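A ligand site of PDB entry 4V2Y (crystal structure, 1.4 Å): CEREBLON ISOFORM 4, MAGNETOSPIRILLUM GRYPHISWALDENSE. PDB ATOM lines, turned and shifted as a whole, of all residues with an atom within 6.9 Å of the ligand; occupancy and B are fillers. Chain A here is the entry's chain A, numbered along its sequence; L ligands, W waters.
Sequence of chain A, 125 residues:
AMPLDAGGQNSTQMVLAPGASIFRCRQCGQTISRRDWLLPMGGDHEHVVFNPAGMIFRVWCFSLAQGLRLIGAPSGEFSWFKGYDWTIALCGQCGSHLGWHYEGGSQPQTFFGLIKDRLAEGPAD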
ATOM      1  N   VAL A  49      -0.696   9.867  -6.404  1.00  0.00           N
ATOM      2  CA  VAL A  49      -0.790  11.157  -7.124  1.00  0.00           C
ATOM      3  C   VAL A  49      -0.531  10.940  -8.593  1.00  0.00           C
ATOM      4  O   VAL A  49       0.037   9.888  -8.955  1.00  0.00           O
ATOM      5  CB  VAL A  49       0.250  12.137  -6.560  1.00  0.00           C
ATOM      6  CG1 VAL A  49      -0.212  12.541  -5.158  1.00  0.00           C
ATOM      7  CG2 VAL A  49       1.669  11.533  -6.611  1.00  0.00           C
ATOM      8  N   PHE A  50      -0.905  11.911  -9.439  1.00  0.00           N
ATOM      9  CA  PHE A  50      -0.580  11.875 -10.894  1.00  0.00           C
ATOM     10  C   PHE A  50       0.107  13.128 -11.339  1.00  0.00           C
ATOM     11  O   PHE A  50      -0.249  14.219 -10.827  1.00  0.00           O
ATOM     12  CB  PHE A  50      -1.851  11.712 -11.807  1.00  0.00           C
ATOM     13  CG  PHE A  50      -2.728  10.592 -11.406  1.00  0.00           C
ATOM     14  CD1 PHE A  50      -3.620  10.770 -10.369  1.00  0.00           C
ATOM     15  CD2 PHE A  50      -2.811   9.483 -12.196  1.00  0.00           C
ATOM     16  CE1 PHE A  50      -4.471   9.763  -9.999  1.00  0.00           C
ATOM     17  CE2 PHE A  50      -3.670   8.425 -11.868  1.00  0.00           C
ATOM     18  CZ  PHE A  50      -4.487   8.575 -10.738  1.00  0.00           C
ATOM     19  N   ASN A  51       1.043  13.008 -12.233  1.00  0.00           N
ATOM     20  CA  ASN A  51       1.642  14.204 -12.865  1.00  0.00           C
ATOM     21  C   ASN A  51       0.903  14.625 -14.101  1.00  0.00           C
ATOM     22  O   ASN A  51      -0.145  14.032 -14.491  1.00  0.00           O
ATOM     23  CB  ASN A  51       3.115  13.960 -13.092  1.00  0.00           C
ATOM     24  CG  ASN A  51       3.413  12.924 -14.188  1.00  0.00           C
ATOM     25  OD1 ASN A  51       2.532  12.566 -14.981  1.00  0.00           O
ATOM     26  ND2 ASN A  51       4.675  12.547 -14.283  1.00  0.00           N
ATOM     27  N   PRO A  52       1.291  15.746 -14.735  1.00  0.00           N
ATOM     28  CA  PRO A  52       0.578  16.211 -15.874  1.00  0.00           C
ATOM     29  C   PRO A  52       0.570  15.271 -17.083  1.00  0.00           C
ATOM     30  O   PRO A  52      -0.337  15.374 -17.957  1.00  0.00           O
ATOM     31  CB  PRO A  52       1.227  17.556 -16.211  1.00  0.00           C
ATOM     32  CG  PRO A  52       1.819  17.974 -14.906  1.00  0.00           C
ATOM     33  CD  PRO A  52       2.230  16.768 -14.192  1.00  0.00           C
ATOM     34  N   ALA A  53       1.468  14.312 -17.047  1.00  0.00           N
ATOM     35  CA  ALA A  53       1.534  13.321 -18.198  1.00  0.00           C
ATOM     36  C   ALA A  53       0.742  12.076 -17.800  1.00  0.00           C
ATOM     37  O   ALA A  53       0.744  11.079 -18.501  1.00  0.00           O
ATOM     38  CB  ALA A  53       2.934  12.938 -18.505  1.00  0.00           C
ATOM     39  N   MET A  55       0.999  10.016 -15.352  1.00  0.00           N
ATOM     40  CA  MET A  55       1.646   8.908 -14.667  1.00  0.00           C
ATOM     41  C   MET A  55       1.228   8.924 -13.227  1.00  0.00           C
ATOM     42  O   MET A  55       1.254  10.005 -12.544  1.00  0.00           O
ATOM     43  CB  MET A  55       3.154   8.992 -14.778  1.00  0.00           C
ATOM     44  CG  MET A  55       3.675   9.078 -16.213  1.00  0.00           C
ATOM     45  SD  MET A  55       5.403   9.580 -16.202  1.00  0.00           S
ATOM     46  CE  MET A  55       6.260   8.014 -16.388  1.00  0.00           C
ATOM     47  N   PHE A  57       1.803   7.759  -9.285  1.00  0.00           N
ATOM     48  CA  PHE A  57       2.901   7.425  -8.388  1.00  0.00           C
ATOM     49  C   PHE A  57       2.332   7.126  -7.017  1.00  0.00           C
ATOM     50  O   PHE A  57       1.533   7.883  -6.481  1.00  0.00           O
ATOM     51  CB  PHE A  57       3.906   8.520  -8.234  1.00  0.00           C
ATOM     52  CG  PHE A  57       4.551   8.988  -9.506  1.00  0.00           C
ATOM     53  CD1 PHE A  57       5.659   8.395 -10.002  1.00  0.00           C
ATOM     54  CD2 PHE A  57       3.995  10.062 -10.231  1.00  0.00           C
ATOM     55  CE1 PHE A  57       6.220   8.798 -11.198  1.00  0.00           C
ATOM     56  CE2 PHE A  57       4.547  10.449 -11.428  1.00  0.00           C
ATOM     57  CZ  PHE A  57       5.675   9.856 -11.884  1.00  0.00           C
ATOM     58  N   SER A  75      10.714  24.158  -7.573  1.00  0.00           N
ATOM     59  CA  SER A  75       9.568  24.622  -8.271  1.00  0.00           C
ATOM     60  C   SER A  75       8.260  24.364  -7.533  1.00  0.00           C
ATOM     61  O   SER A  75       8.129  23.241  -6.980  1.00  0.00           O
ATOM     62  CB  SER A  75       9.475  23.957  -9.633  1.00  0.00           C
ATOM     63  OG  SER A  75       8.365  24.438 -10.293  1.00  0.00           O
ATOM     64  N   GLY A  76       7.341  25.266  -7.544  1.00  0.00           N
ATOM     65  CA  GLY A  76       6.031  25.022  -6.990  1.00  0.00           C
ATOM     66  C   GLY A  76       5.025  24.416  -7.954  1.00  0.00           C
ATOM     67  O   GLY A  76       3.938  24.123  -7.574  1.00  0.00           O
ATOM     68  N   GLU A  77       5.390  24.378  -9.234  1.00  0.00           N
ATOM     69  CA  GLU A  77       4.412  24.031 -10.268  1.00  0.00           C
ATOM     70  C   GLU A  77       3.956  22.616 -10.038  1.00  0.00           C
ATOM     71  O   GLU A  77       4.706  21.688  -9.869  1.00  0.00           O
ATOM     72  CB  GLU A  77       5.101  24.144 -11.601  1.00  0.00           C
ATOM     73  CG  GLU A  77       5.381  25.601 -11.894  1.00  0.00           C
ATOM     74  CD  GLU A  77       6.003  25.829 -13.237  1.00  0.00           C
ATOM     75  OE1 GLU A  77       6.214  24.853 -13.965  1.00  0.00           O
ATOM     76  OE2 GLU A  77       6.283  27.003 -13.529  1.00  0.00           O
ATOM     77  N   PHE A  78       2.630  22.477 -10.072  1.00  0.00           N
ATOM     78  CA  PHE A  78       1.989  21.167 -10.003  1.00  0.00           C
ATOM     79  C   PHE A  78       2.184  20.483  -8.683  1.00  0.00           C
ATOM     80  O   PHE A  78       2.042  19.301  -8.578  1.00  0.00           O
ATOM     81  CB  PHE A  78       2.345  20.236 -11.161  1.00  0.00           C
ATOM     82  CG  PHE A  78       2.038  20.819 -12.507  1.00  0.00           C
ATOM     83  CD1 PHE A  78       0.767  21.025 -12.887  1.00  0.00           C
ATOM     84  CD2 PHE A  78       3.077  21.166 -13.356  1.00  0.00           C
ATOM     85  CE1 PHE A  78       0.468  21.563 -14.144  1.00  0.00           C
ATOM     86  CE2 PHE A  78       2.784  21.726 -14.590  1.00  0.00           C
ATOM     87  CZ  PHE A  78       1.519  21.871 -14.989  1.00  0.00           C
ATOM     88  N   SER A  79       2.707  21.181  -7.635  1.00  0.00           N
ATOM     89  CA  SER A  79       3.041  20.485  -6.384  1.00  0.00           C
ATOM     90  C   SER A  79       1.840  19.777  -5.789  1.00  0.00           C
ATOM     91  O   SER A  79       0.753  20.339  -5.662  1.00  0.00           O
ATOM     92  CB  SER A  79       3.575  21.475  -5.357  1.00  0.00           C
ATOM     93  OG  SER A  79       3.992  20.729  -4.217  1.00  0.00           O
ATOM     94  N   TRP A  80       2.103  18.495  -5.441  1.00  0.00           N
ATOM     95  CA  TRP A  80       1.108  17.651  -4.794  1.00  0.00           C
ATOM     96  C   TRP A  80       0.887  17.978  -3.312  1.00  0.00           C
ATOM     97  O   TRP A  80      -0.084  17.580  -2.721  1.00  0.00           O
ATOM     98  CB  TRP A  80       1.497  16.190  -4.909  1.00  0.00           C
ATOM     99  CG  TRP A  80       1.519  15.668  -6.291  1.00  0.00           C
ATOM    100  CD1 TRP A  80       0.543  15.857  -7.195  1.00  0.00           C
ATOM    101  CD2 TRP A  80       2.560  14.968  -6.885  1.00  0.00           C
ATOM    102  NE1 TRP A  80       0.911  15.191  -8.454  1.00  0.00           N
ATOM    103  CE2 TRP A  80       2.123  14.633  -8.229  1.00  0.00           C
ATOM    104  CE3 TRP A  80       3.784  14.454  -6.450  1.00  0.00           C
ATOM    105  CZ2 TRP A  80       2.981  13.906  -9.072  1.00  0.00           C
ATOM    106  CZ3 TRP A  80       4.542  13.735  -7.284  1.00  0.00           C
ATOM    107  CH2 TRP A  80       4.149  13.446  -8.585  1.00  0.00           C
ATOM    108  N   PHE A  81       1.745  18.799  -2.731  1.00  0.00           N
ATOM    109  CA  PHE A  81       1.732  19.054  -1.277  1.00  0.00           C
ATOM    110  C   PHE A  81       1.649  20.572  -1.067  1.00  0.00           C
ATOM    111  O   PHE A  81       2.568  21.286  -1.444  1.00  0.00           O
ATOM    112  CB  PHE A  81       2.934  18.454  -0.579  1.00  0.00           C
ATOM    113  CG  PHE A  81       3.029  16.930  -0.719  1.00  0.00           C
ATOM    114  CD1 PHE A  81       2.354  16.110   0.199  1.00  0.00           C
ATOM    115  CD2 PHE A  81       3.737  16.368  -1.696  1.00  0.00           C
ATOM    116  CE1 PHE A  81       2.463  14.706   0.123  1.00  0.00           C
ATOM    117  CE2 PHE A  81       3.829  14.967  -1.874  1.00  0.00           C
ATOM    118  CZ  PHE A  81       3.179  14.157  -0.923  1.00  0.00           C
ATOM    119  N   TYR A  84       4.546  23.500  -0.513  1.00  0.00           N
ATOM    120  CA  TYR A  84       5.850  22.962  -0.791  1.00  0.00           C
ATOM    121  C   TYR A  84       6.305  23.091  -2.223  1.00  0.00           C
ATOM    122  O   TYR A  84       5.467  22.923  -3.139  1.00  0.00           O
ATOM    123  CB  TYR A  84       6.043  21.475  -0.361  1.00  0.00           C
ATOM    124  CG  TYR A  84       5.800  21.185   1.074  1.00  0.00           C
ATOM    125  CD1 TYR A  84       4.585  20.932   1.587  1.00  0.00           C
ATOM    126  CD2 TYR A  84       6.870  21.235   1.965  1.00  0.00           C
ATOM    127  CE1 TYR A  84       4.395  20.664   2.957  1.00  0.00           C
ATOM    128  CE2 TYR A  84       6.712  20.948   3.274  1.00  0.00           C
ATOM    129  CZ  TYR A  84       5.480  20.690   3.795  1.00  0.00           C
ATOM    130  OH  TYR A  84       5.181  20.465   5.124  1.00  0.00           O
ATOM    131  N   TRP A  86       9.298  21.641  -4.978  1.00  0.00           N
ATOM    132  CA  TRP A  86      10.016  20.375  -5.182  1.00  0.00           C
ATOM    133  C   TRP A  86      11.226  20.461  -6.068  1.00  0.00           C
ATOM    134  O   TRP A  86      11.280  21.321  -6.955  1.00  0.00           O
ATOM    135  CB  TRP A  86       9.041  19.347  -5.733  1.00  0.00           C
ATOM    136  CG  TRP A  86       8.315  19.712  -6.947  1.00  0.00           C
ATOM    137  CD1 TRP A  86       7.062  20.276  -7.043  1.00  0.00           C
ATOM    138  CD2 TRP A  86       8.838  19.700  -8.309  1.00  0.00           C
ATOM    139  NE1 TRP A  86       6.779  20.566  -8.344  1.00  0.00           N
ATOM    140  CE2 TRP A  86       7.842  20.258  -9.143  1.00  0.00           C
ATOM    141  CE3 TRP A  86       9.992  19.197  -8.926  1.00  0.00           C
ATOM    142  CZ2 TRP A  86       7.997  20.400 -10.508  1.00  0.00           C
ATOM    143  CZ3 TRP A  86      10.158  19.394 -10.310  1.00  0.00           C
ATOM    144  CH2 TRP A  86       9.107  19.919 -11.108  1.00  0.00           C
ATOM    145  N   THR A  87      12.141  19.486  -5.842  1.00  0.00           N
ATOM    146  CA  THR A  87      13.279  19.208  -6.706  1.00  0.00           C
ATOM    147  C   THR A  87      13.188  17.722  -6.975  1.00  0.00           C
ATOM    148  O   THR A  87      12.901  16.924  -6.092  1.00  0.00           O
ATOM    149  CB  THR A  87      14.634  19.573  -6.126  1.00  0.00           C
ATOM    150  OG1 THR A  87      14.856  18.903  -4.928  1.00  0.00           O
ATOM    151  CG2 THR A  87      14.577  21.042  -5.701  1.00  0.00           C
ATOM    152  N   ILE A  88      13.508  17.349  -8.187  1.00  0.00           N
ATOM    153  CA  ILE A  88      13.690  15.916  -8.594  1.00  0.00           C
ATOM    154  C   ILE A  88      14.774  15.287  -7.709  1.00  0.00           C
ATOM    155  O   ILE A  88      15.875  15.892  -7.603  1.00  0.00           O
ATOM    156  CB  ILE A  88      13.982  15.854 -10.082  1.00  0.00           C
ATOM    157  CG1 ILE A  88      12.731  16.148 -10.820  1.00  0.00           C
ATOM    158  CG2 ILE A  88      14.511  14.462 -10.459  1.00  0.00           C
ATOM    159  CD1 ILE A  88      12.872  16.335 -12.332  1.00  0.00           C
ATOM    160  N   HIS A  97      15.106   7.691 -11.195  1.00  0.00           N
ATOM    161  CA  HIS A  97      14.284   8.706 -10.580  1.00  0.00           C
ATOM    162  C   HIS A  97      13.529   8.129  -9.425  1.00  0.00           C
ATOM    163  O   HIS A  97      12.591   7.306  -9.563  1.00  0.00           O
ATOM    164  CB  HIS A  97      13.308   9.271 -11.579  1.00  0.00           C
ATOM    165  CG  HIS A  97      12.405  10.271 -10.974  1.00  0.00           C
ATOM    166  ND1 HIS A  97      11.151  10.539 -11.521  1.00  0.00           N
ATOM    167  CD2 HIS A  97      12.546  11.097  -9.922  1.00  0.00           C
ATOM    168  CE1 HIS A  97      10.589  11.475 -10.785  1.00  0.00           C
ATOM    169  NE2 HIS A  97      11.401  11.811  -9.815  1.00  0.00           N
ATOM    170  N   TRP A 100      11.119  12.909  -5.130  1.00  0.00           N
ATOM    171  CA  TRP A 100      11.281  14.395  -5.041  1.00  0.00           C
ATOM    172  C   TRP A 100      11.640  14.767  -3.628  1.00  0.00           C
ATOM    173  O   TRP A 100      11.219  14.107  -2.648  1.00  0.00           O
ATOM    174  CB  TRP A 100       9.967  15.092  -5.429  1.00  0.00           C
ATOM    175  CG  TRP A 100       9.492  14.756  -6.829  1.00  0.00           C
ATOM    176  CD1 TRP A 100       9.791  15.430  -7.983  1.00  0.00           C
ATOM    177  CD2 TRP A 100       8.693  13.639  -7.224  1.00  0.00           C
ATOM    178  NE1 TRP A 100       9.258  14.778  -9.050  1.00  0.00           N
ATOM    179  CE2 TRP A 100       8.567  13.699  -8.621  1.00  0.00           C
ATOM    180  CE3 TRP A 100       8.077  12.580  -6.537  1.00  0.00           C
ATOM    181  CZ2 TRP A 100       7.801  12.746  -9.333  1.00  0.00           C
ATOM    182  CZ3 TRP A 100       7.431  11.571  -7.289  1.00  0.00           C
ATOM    183  CH2 TRP A 100       7.308  11.718  -8.636  1.00  0.00           C
ATOM    184  N   TYR A 102      10.973  17.921  -1.119  1.00  0.00           N
ATOM    185  CA  TYR A 102      10.073  19.039  -0.893  1.00  0.00           C
ATOM    186  C   TYR A 102      10.651  20.003   0.165  1.00  0.00           C
ATOM    187  O   TYR A 102      11.215  19.558   1.148  1.00  0.00           O
ATOM    188  CB  TYR A 102       8.708  18.540  -0.484  1.00  0.00           C
ATOM    189  CG  TYR A 102       7.969  17.825  -1.586  1.00  0.00           C
ATOM    190  CD1 TYR A 102       7.246  18.561  -2.492  1.00  0.00           C
ATOM    191  CD2 TYR A 102       8.083  16.465  -1.768  1.00  0.00           C
ATOM    192  CE1 TYR A 102       6.573  17.956  -3.520  1.00  0.00           C
ATOM    193  CE2 TYR A 102       7.427  15.832  -2.800  1.00  0.00           C
ATOM    194  CZ  TYR A 102       6.730  16.601  -3.708  1.00  0.00           C
ATOM    195  OH  TYR A 102       6.049  15.954  -4.748  1.00  0.00           O
HETATM  196  O1  LIG L   1       3.324  16.745 -10.883  1.00  0.00           O
HETATM  197  C1  LIG L   1       4.314  16.803 -10.038  1.00  0.00           C
HETATM  198  N1  LIG L   1       4.086  17.285  -8.819  1.00  0.00           N
HETATM  199  C2  LIG L   1       5.040  17.241  -7.863  1.00  0.00           C
HETATM  200  O2  LIG L   1       4.697  17.543  -6.665  1.00  0.00           O
HETATM  201  C3  LIG L   1       6.418  16.818  -8.260  1.00  0.00           C
HETATM  202  C4  LIG L   1       6.729  16.967  -9.720  1.00  0.00           C
HETATM  203  C5  LIG L   1       5.627  16.289 -10.519  1.00  0.00           C
HETATM  204  N2  LIG L   1       5.898  16.478 -11.949  1.00  0.00           N
HETATM  205  C6  LIG L   1       6.230  17.539 -16.442  1.00  0.00           C
HETATM  206  C7  LIG L   1       5.939  18.126 -15.206  1.00  0.00           C
HETATM  207  C8  LIG L   1       5.984  17.320 -14.088  1.00  0.00           C
HETATM  208  C9  LIG L   1       6.238  15.987 -14.134  1.00  0.00           C
HETATM  209  O3  LIG L   1       5.439  18.775 -12.123  1.00  0.00           O
HETATM  210  O4  LIG L   1       6.287  14.238 -12.402  1.00  0.00           O
HETATM  211  C10 LIG L   1       6.470  15.391 -15.356  1.00  0.00           C
HETATM  212  C11 LIG L   1       6.476  16.177 -16.495  1.00  0.00           C
HETATM  213  C12 LIG L   1       6.180  15.515 -12.852  1.00  0.00           C
HETATM  214  C13 LIG L   1       5.714  17.565 -12.652  1.00  0.00           C
HETATM  215  O   HOH W   1       9.414  15.645 -11.945  1.00  0.00           O
HETATM  216  O   HOH W   2       6.643  20.974 -13.562  1.00  0.00           O
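Water W1 lies within hydrogen-bond range of the indole nitrogen (NE1) of Trp 100 (3.0 Å) and an oxygen (O4) of the ligand (3.5 Å).
Pro 52 touches the ligand. Glu 77 touches the ligand (O to O3, 3.8 Å). Ser 79 touches the ligand (CA to O2, 3.4 Å). Trp 86 touches the ligand. Trp 100 touches the ligand (NE1 to C4, 3.4 Å). Nine residues have an atom within 4 Å of the ligand: Asn 51, Pro 52, Glu 77, Phe 78, Ser 79, Trp 80, Trp 86, Trp 100 and Tyr 102. The nearest printed residue that does not touch the ligand is Phe 57 (4.3 Å).
The backbone NH of Ala 53 is in hydrogen-bond range of the side-chain amide oxygen of Asn 51 (2.9 Å). The side-chain amide oxygen of Asn 51 is in hydrogen-bond range of the backbone NH of Met 55, at 3.0 Å. O of Phe 50 sits at hydrogen-bond distance from NE1 of Trp 80, 2.8 Å away. O of Phe 81 sits at hydrogen-bond distance from OG of Ser 79 (3.2 Å). The backbone carbonyl oxygen (O) of Tyr 84 is in hydrogen-bond range of the side-chain hydroxyl (OG) of Ser 79. NE1 of Trp 86 lies within hydrogen-bond range of O of Glu 77, at 2.8 Å. O of Ser 75 lies within hydrogen-bond range of N of Trp 86 (2.8 Å). The backbone NH (N) of Glu 77 sits at hydrogen-bond distance from the side-chain hydroxyl (OG) of Ser 75 (3.2 Å).
The side-chain hydroxyl (OH) of Tyr 102 is in hydrogen-bond range of an oxygen (O2) of the ligand, at 2.8 Å. The backbone carbonyl oxygen (O) of Phe 78 is in hydrogen-bond range of a nitrogen (N1) of the ligand. O4 of the ligand is in hydrogen-bond range of ND2 of Asn 51, 3.0 Å away. The backbone NH (N) of Trp 80 is in hydrogen-bond range of an oxygen (O2) of the ligand (3.0 Å).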
